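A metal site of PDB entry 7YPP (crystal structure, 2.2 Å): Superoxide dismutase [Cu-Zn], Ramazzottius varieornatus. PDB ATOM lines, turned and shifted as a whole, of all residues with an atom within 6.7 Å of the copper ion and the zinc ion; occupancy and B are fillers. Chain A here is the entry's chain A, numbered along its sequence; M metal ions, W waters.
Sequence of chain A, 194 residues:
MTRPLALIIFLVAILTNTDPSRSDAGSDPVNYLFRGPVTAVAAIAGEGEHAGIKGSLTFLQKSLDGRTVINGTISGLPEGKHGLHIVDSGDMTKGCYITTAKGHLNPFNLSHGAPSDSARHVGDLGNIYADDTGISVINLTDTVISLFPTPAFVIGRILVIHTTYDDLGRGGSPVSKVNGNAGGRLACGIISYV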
ATOM      1  N   GLY A  83     -11.778  25.382  -3.731  1.00  0.00           N
ATOM      2  CA  GLY A  83     -11.557  25.158  -2.319  1.00  0.00           C
ATOM      3  C   GLY A  83     -12.778  25.601  -1.501  1.00  0.00           C
ATOM      4  O   GLY A  83     -13.338  26.679  -1.730  1.00  0.00           O
ATOM      5  N   LEU A  84     -13.161  24.755  -0.546  1.00  0.00           N
ATOM      6  CA  LEU A  84     -14.260  25.039   0.358  1.00  0.00           C
ATOM      7  C   LEU A  84     -13.708  25.055   1.784  1.00  0.00           C
ATOM      8  O   LEU A  84     -13.319  24.014   2.304  1.00  0.00           O
ATOM      9  CB  LEU A  84     -15.319  23.955   0.172  1.00  0.00           C
ATOM     10  CG  LEU A  84     -16.607  24.122   0.976  1.00  0.00           C
ATOM     11  CD1 LEU A  84     -17.441  25.291   0.442  1.00  0.00           C
ATOM     12  CD2 LEU A  84     -17.384  22.815   0.983  1.00  0.00           C
ATOM     13  N   HIS A  85     -13.640  26.227   2.400  1.00  0.00           N
ATOM     14  CA  HIS A  85     -12.950  26.347   3.670  1.00  0.00           C
ATOM     15  C   HIS A  85     -13.760  27.189   4.650  1.00  0.00           C
ATOM     16  O   HIS A  85     -14.480  28.101   4.251  1.00  0.00           O
ATOM     17  CB  HIS A  85     -11.571  26.986   3.504  1.00  0.00           C
ATOM     18  CG  HIS A  85     -10.668  26.284   2.543  1.00  0.00           C
ATOM     19  ND1 HIS A  85      -9.785  26.997   1.726  1.00  0.00           N
ATOM     20  CD2 HIS A  85     -10.497  24.980   2.229  1.00  0.00           C
ATOM     21  CE1 HIS A  85      -9.101  26.151   0.994  1.00  0.00           C
ATOM     22  NE2 HIS A  85      -9.508  24.909   1.283  1.00  0.00           N
ATOM     23  N   ILE A  86     -13.614  26.872   5.948  1.00  0.00           N
ATOM     24  CA  ILE A  86     -14.186  27.673   7.003  1.00  0.00           C
ATOM     25  C   ILE A  86     -13.056  28.513   7.591  1.00  0.00           C
ATOM     26  O   ILE A  86     -12.044  27.948   7.990  1.00  0.00           O
ATOM     27  CB  ILE A  86     -14.902  26.792   8.052  1.00  0.00           C
ATOM     28  CG1 ILE A  86     -15.934  25.858   7.397  1.00  0.00           C
ATOM     29  CG2 ILE A  86     -15.539  27.641   9.142  1.00  0.00           C
ATOM     30  CD1 ILE A  86     -16.522  24.826   8.341  1.00  0.00           C
ATOM     31  N   VAL A  87     -13.213  29.845   7.628  1.00  0.00           N
ATOM     32  CA  VAL A  87     -12.168  30.736   8.133  1.00  0.00           C
ATOM     33  C   VAL A  87     -12.422  31.052   9.607  1.00  0.00           C
ATOM     34  O   VAL A  87     -13.481  30.706  10.136  1.00  0.00           O
ATOM     35  CB  VAL A  87     -11.996  32.015   7.274  1.00  0.00           C
ATOM     36  CG1 VAL A  87     -11.446  31.695   5.905  1.00  0.00           C
ATOM     37  CG2 VAL A  87     -13.294  32.805   7.168  1.00  0.00           C
ATOM     38  N   HIS A 104      -7.609  29.952   8.047  1.00  0.00           N
ATOM     39  CA  HIS A 104      -8.598  28.905   8.213  1.00  0.00           C
ATOM     40  C   HIS A 104      -8.888  28.661   9.700  1.00  0.00           C
ATOM     41  O   HIS A 104      -7.985  28.786  10.519  1.00  0.00           O
ATOM     42  CB  HIS A 104      -8.141  27.611   7.530  1.00  0.00           C
ATOM     43  CG  HIS A 104      -8.044  27.730   6.055  1.00  0.00           C
ATOM     44  ND1 HIS A 104      -7.479  26.739   5.277  1.00  0.00           N
ATOM     45  CD2 HIS A 104      -8.399  28.745   5.220  1.00  0.00           C
ATOM     46  CE1 HIS A 104      -7.517  27.109   4.013  1.00  0.00           C
ATOM     47  NE2 HIS A 104      -8.061  28.338   3.944  1.00  0.00           N
ATOM     48  N   LEU A 105     -10.124  28.266  10.013  1.00  0.00           N
ATOM     49  CA  LEU A 105     -10.484  27.884  11.377  1.00  0.00           C
ATOM     50  C   LEU A 105      -9.567  26.754  11.848  1.00  0.00           C
ATOM     51  O   LEU A 105      -9.590  25.667  11.281  1.00  0.00           O
ATOM     52  CB  LEU A 105     -11.962  27.486  11.407  1.00  0.00           C
ATOM     53  CG  LEU A 105     -12.522  27.164  12.802  1.00  0.00           C
ATOM     54  CD1 LEU A 105     -12.422  28.371  13.725  1.00  0.00           C
ATOM     55  CD2 LEU A 105     -13.935  26.609  12.753  1.00  0.00           C
ATOM     56  N   SER A 111      -1.386  22.098  10.574  1.00  0.00           N
ATOM     57  CA  SER A 111      -1.136  22.640   9.253  1.00  0.00           C
ATOM     58  C   SER A 111      -2.323  22.312   8.322  1.00  0.00           C
ATOM     59  O   SER A 111      -3.175  21.515   8.666  1.00  0.00           O
ATOM     60  CB  SER A 111       0.180  22.150   8.690  1.00  0.00           C
ATOM     61  OG  SER A 111       0.194  20.734   8.697  1.00  0.00           O
ATOM     62  N   HIS A 112      -2.360  22.959   7.160  1.00  0.00           N
ATOM     63  CA  HIS A 112      -3.417  22.773   6.183  1.00  0.00           C
ATOM     64  C   HIS A 112      -3.273  21.397   5.524  1.00  0.00           C
ATOM     65  O   HIS A 112      -2.169  20.971   5.175  1.00  0.00           O
ATOM     66  CB  HIS A 112      -3.390  23.877   5.122  1.00  0.00           C
ATOM     67  CG  HIS A 112      -4.444  23.714   4.083  1.00  0.00           C
ATOM     68  ND1 HIS A 112      -5.739  24.124   4.285  1.00  0.00           N
ATOM     69  CD2 HIS A 112      -4.416  23.142   2.857  1.00  0.00           C
ATOM     70  CE1 HIS A 112      -6.469  23.829   3.225  1.00  0.00           C
ATOM     71  NE2 HIS A 112      -5.684  23.227   2.331  1.00  0.00           N
ATOM     72  N   GLY A 113      -4.419  20.703   5.341  1.00  0.00           N
ATOM     73  CA  GLY A 113      -4.422  19.452   4.591  1.00  0.00           C
ATOM     74  C   GLY A 113      -5.771  19.189   3.939  1.00  0.00           C
ATOM     75  O   GLY A 113      -6.663  20.029   3.990  1.00  0.00           O
ATOM     76  N   ARG A 120      -4.730  18.658   9.544  1.00  0.00           N
ATOM     77  CA  ARG A 120      -5.644  19.535   8.818  1.00  0.00           C
ATOM     78  C   ARG A 120      -6.221  20.561   9.777  1.00  0.00           C
ATOM     79  O   ARG A 120      -6.167  20.371  10.986  1.00  0.00           O
ATOM     80  CB  ARG A 120      -6.802  18.752   8.178  1.00  0.00           C
ATOM     81  CG  ARG A 120      -7.631  17.956   9.175  1.00  0.00           C
ATOM     82  CD  ARG A 120      -8.959  17.524   8.592  1.00  0.00           C
ATOM     83  NE  ARG A 120      -9.971  18.558   8.676  1.00  0.00           N
ATOM     84  CZ  ARG A 120     -11.265  18.366   8.445  1.00  0.00           C
ATOM     85  NH1 ARG A 120     -11.703  17.158   8.090  1.00  0.00           N
ATOM     86  NH2 ARG A 120     -12.111  19.371   8.591  1.00  0.00           N
ATOM     87  N   HIS A 121      -6.731  21.660   9.218  1.00  0.00           N
ATOM     88  CA  HIS A 121      -7.518  22.636   9.954  1.00  0.00           C
ATOM     89  C   HIS A 121      -8.939  22.119  10.126  1.00  0.00           C
ATOM     90  O   HIS A 121      -9.394  21.331   9.298  1.00  0.00           O
ATOM     91  CB  HIS A 121      -7.542  23.963   9.207  1.00  0.00           C
ATOM     92  CG  HIS A 121      -6.191  24.524   8.929  1.00  0.00           C
ATOM     93  ND1 HIS A 121      -5.861  25.081   7.708  1.00  0.00           N
ATOM     94  CD2 HIS A 121      -5.081  24.616   9.704  1.00  0.00           C
ATOM     95  CE1 HIS A 121      -4.623  25.504   7.747  1.00  0.00           C
ATOM     96  NE2 HIS A 121      -4.118  25.235   8.956  1.00  0.00           N
ATOM     97  N   VAL A 122      -9.623  22.567  11.189  1.00  0.00           N
ATOM     98  CA  VAL A 122     -11.039  22.256  11.326  1.00  0.00           C
ATOM     99  C   VAL A 122     -11.747  22.693  10.050  1.00  0.00           C
ATOM    100  O   VAL A 122     -12.619  21.988   9.551  1.00  0.00           O
ATOM    101  CB  VAL A 122     -11.648  22.892  12.589  1.00  0.00           C
ATOM    102  CG1 VAL A 122     -13.180  22.846  12.550  1.00  0.00           C
ATOM    103  CG2 VAL A 122     -11.178  22.205  13.852  1.00  0.00           C
ATOM    104  N   GLY A 123     -11.322  23.847   9.502  1.00  0.00           N
ATOM    105  CA  GLY A 123     -12.011  24.499   8.400  1.00  0.00           C
ATOM    106  C   GLY A 123     -11.709  23.901   7.021  1.00  0.00           C
ATOM    107  O   GLY A 123     -12.184  24.438   6.012  1.00  0.00           O
ATOM    108  N   ASP A 124     -10.938  22.805   6.972  1.00  0.00           N
ATOM    109  CA  ASP A 124     -10.480  22.253   5.712  1.00  0.00           C
ATOM    110  C   ASP A 124     -11.494  21.242   5.181  1.00  0.00           C
ATOM    111  O   ASP A 124     -11.422  20.046   5.529  1.00  0.00           O
ATOM    112  CB  ASP A 124      -9.099  21.598   5.859  1.00  0.00           C
ATOM    113  CG  ASP A 124      -7.984  22.600   6.145  1.00  0.00           C
ATOM    114  OD1 ASP A 124      -8.243  23.810   6.012  1.00  0.00           O
ATOM    115  OD2 ASP A 124      -6.860  22.152   6.502  1.00  0.00           O
ATOM    116  N   VAL A 160     -16.102  29.744   2.903  1.00  0.00           N
ATOM    117  CA  VAL A 160     -15.583  30.434   1.729  1.00  0.00           C
ATOM    118  C   VAL A 160     -15.531  29.456   0.559  1.00  0.00           C
ATOM    119  O   VAL A 160     -15.141  28.303   0.743  1.00  0.00           O
ATOM    120  CB  VAL A 160     -14.194  31.027   2.041  1.00  0.00           C
ATOM    121  CG1 VAL A 160     -13.441  31.373   0.782  1.00  0.00           C
ATOM    122  CG2 VAL A 160     -14.280  32.252   2.945  1.00  0.00           C
ATOM    123  N   HIS A 162     -13.449  29.296  -2.880  1.00  0.00           N
ATOM    124  CA  HIS A 162     -12.251  29.945  -3.407  1.00  0.00           C
ATOM    125  C   HIS A 162     -12.285  30.040  -4.935  1.00  0.00           C
ATOM    126  O   HIS A 162     -12.991  29.280  -5.612  1.00  0.00           O
ATOM    127  CB  HIS A 162     -10.992  29.210  -2.926  1.00  0.00           C
ATOM    128  CG  HIS A 162     -10.564  29.621  -1.563  1.00  0.00           C
ATOM    129  ND1 HIS A 162      -9.866  30.782  -1.317  1.00  0.00           N
ATOM    130  CD2 HIS A 162     -10.726  29.035  -0.371  1.00  0.00           C
ATOM    131  CE1 HIS A 162      -9.612  30.894  -0.023  1.00  0.00           C
ATOM    132  NE2 HIS A 162     -10.135  29.843   0.570  1.00  0.00           N
ATOM    133  N   ASP A 166      -8.096  23.791  -4.015  1.00  0.00           N
ATOM    134  CA  ASP A 166      -7.218  23.577  -2.887  1.00  0.00           C
ATOM    135  C   ASP A 166      -6.224  22.484  -3.267  1.00  0.00           C
ATOM    136  O   ASP A 166      -6.651  21.430  -3.736  1.00  0.00           O
ATOM    137  CB  ASP A 166      -8.088  23.157  -1.689  1.00  0.00           C
ATOM    138  CG  ASP A 166      -7.352  22.883  -0.387  1.00  0.00           C
ATOM    139  OD1 ASP A 166      -6.095  22.851  -0.369  1.00  0.00           O
ATOM    140  OD2 ASP A 166      -8.065  22.687   0.624  1.00  0.00           O
ATOM    141  N   LYS A 177       0.826  24.696   2.764  1.00  0.00           N
ATOM    142  CA  LYS A 177       0.622  24.161   4.100  1.00  0.00           C
ATOM    143  C   LYS A 177      -0.088  25.200   4.963  1.00  0.00           C
ATOM    144  O   LYS A 177      -0.413  24.943   6.133  1.00  0.00           O
ATOM    145  CB  LYS A 177       1.968  23.730   4.711  1.00  0.00           C
ATOM    146  CG  LYS A 177       2.638  22.516   4.066  1.00  0.00           C
ATOM    147  CD  LYS A 177       1.889  21.225   4.300  1.00  0.00           C
ATOM    148  CE  LYS A 177       2.709  19.993   3.952  1.00  0.00           C
ATOM    149  NZ  LYS A 177       1.838  18.872   3.532  1.00  0.00           N
ATOM    150  N   VAL A 178      -0.338  26.378   4.386  1.00  0.00           N
ATOM    151  CA  VAL A 178      -1.075  27.419   5.081  1.00  0.00           C
ATOM    152  C   VAL A 178      -2.547  27.374   4.671  1.00  0.00           C
ATOM    153  O   VAL A 178      -3.426  27.324   5.541  1.00  0.00           O
ATOM    154  CB  VAL A 178      -0.444  28.818   4.885  1.00  0.00           C
ATOM    155  CG1 VAL A 178      -1.252  29.941   5.532  1.00  0.00           C
ATOM    156  CG2 VAL A 178       0.993  28.846   5.422  1.00  0.00           C
ATOM    157  N   ASN A 179      -2.848  27.340   3.367  1.00  0.00           N
ATOM    158  CA  ASN A 179      -4.232  27.456   2.955  1.00  0.00           C
ATOM    159  C   ASN A 179      -4.531  26.701   1.661  1.00  0.00           C
ATOM    160  O   ASN A 179      -5.638  26.817   1.144  1.00  0.00           O
ATOM    161  CB  ASN A 179      -4.670  28.917   2.816  1.00  0.00           C
ATOM    162  CG  ASN A 179      -3.760  29.705   1.900  1.00  0.00           C
ATOM    163  OD1 ASN A 179      -3.405  29.239   0.808  1.00  0.00           O
ATOM    164  ND2 ASN A 179      -3.339  30.867   2.362  1.00  0.00           N
ATOM    165  N   GLY A 180      -3.561  25.941   1.140  1.00  0.00           N
ATOM    166  CA  GLY A 180      -3.787  25.111  -0.026  1.00  0.00           C
ATOM    167  C   GLY A 180      -3.715  25.872  -1.351  1.00  0.00           C
ATOM    168  O   GLY A 180      -4.084  25.329  -2.389  1.00  0.00           O
ATOM    169  N   ALA A 182      -5.447  28.263  -2.800  1.00  0.00           N
ATOM    170  CA  ALA A 182      -6.701  28.172  -3.527  1.00  0.00           C
ATOM    171  C   ALA A 182      -7.106  29.535  -4.067  1.00  0.00           C
ATOM    172  O   ALA A 182      -8.161  29.675  -4.683  1.00  0.00           O
ATOM    173  CB  ALA A 182      -7.769  27.550  -2.653  1.00  0.00           C
ATOM    174  N   GLY A 183      -6.241  30.541  -3.841  1.00  0.00           N
ATOM    175  CA  GLY A 183      -6.448  31.866  -4.393  1.00  0.00           C
ATOM    176  C   GLY A 183      -7.443  32.679  -3.569  1.00  0.00           C
ATOM    177  O   GLY A 183      -7.644  32.436  -2.376  1.00  0.00           O
HETATM  178 CU    CU M   1      -9.089  28.756   2.193  1.00  0.00          CU
HETATM  179 ZN    ZN M   2      -6.690  24.912   5.964  1.00  0.00          ZN
HETATM  180  O   HOH W   1      -6.753  28.837   0.241  1.00  0.00           O
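OD2 of Asp 124 sits at hydrogen-bond distance from N of Gly 113, at 3.1 Å. The guanidinium group (NH2) of Arg 120 is in hydrogen-bond range of the backbone carbonyl oxygen (O) of Asp 124, 3.2 Å away. The backbone carbonyl oxygen (O) of His 85 is in hydrogen-bond range of the backbone NH (N) of Val 160, at 2.7 Å. The side-chain carboxylate (OD2) of Asp 166 sits at hydrogen-bond distance from a ring nitrogen (NE2) of His 85 (2.7 Å). NE2 of His 112 lies within hydrogen-bond range of OD1 of Asp 166 (2.8 Å). O of Lys 177 sits at hydrogen-bond distance from N of His 112 (3.0 Å). A ring nitrogen (ND1) of His 162 sits at hydrogen-bond distance from the backbone carbonyl oxygen (O) of Gly 183, at 3.0 Å. The backbone NH of His 162 lies within hydrogen-bond range of the backbone carbonyl oxygen of Gly 83 (2.9 Å).
A ring nitrogen (ND1) of His 85 binds the copper ion. A ring nitrogen (NE2) of His 104 is bound to the copper ion (2.1 Å). The copper ion is bound by NE2 of His 162, 2.2 Å away. The copper ion has three donor atoms within binding distance.
Within 4 Å of the zinc ion: His 104, His 112, His 121 and Asp 124.
The zinc ion is bound by OD1 of Asp 124. ND1 of His 121 binds the zinc ion (1.9 Å). ND1 of His 112 binds the zinc ion (2.1 Å). ND1 of His 104 is bound to the zinc ion (2.1 Å). Slightly farther from the zinc ion lies the side-chain carboxylate (OD2) of Asp 124 (2.8 Å).
Three residues have an atom within 4 Å of the copper ion: His 85, His 104 and His 162. The nearest printed residue that does not touch the copper ion is Asn 179 (4.1 Å).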
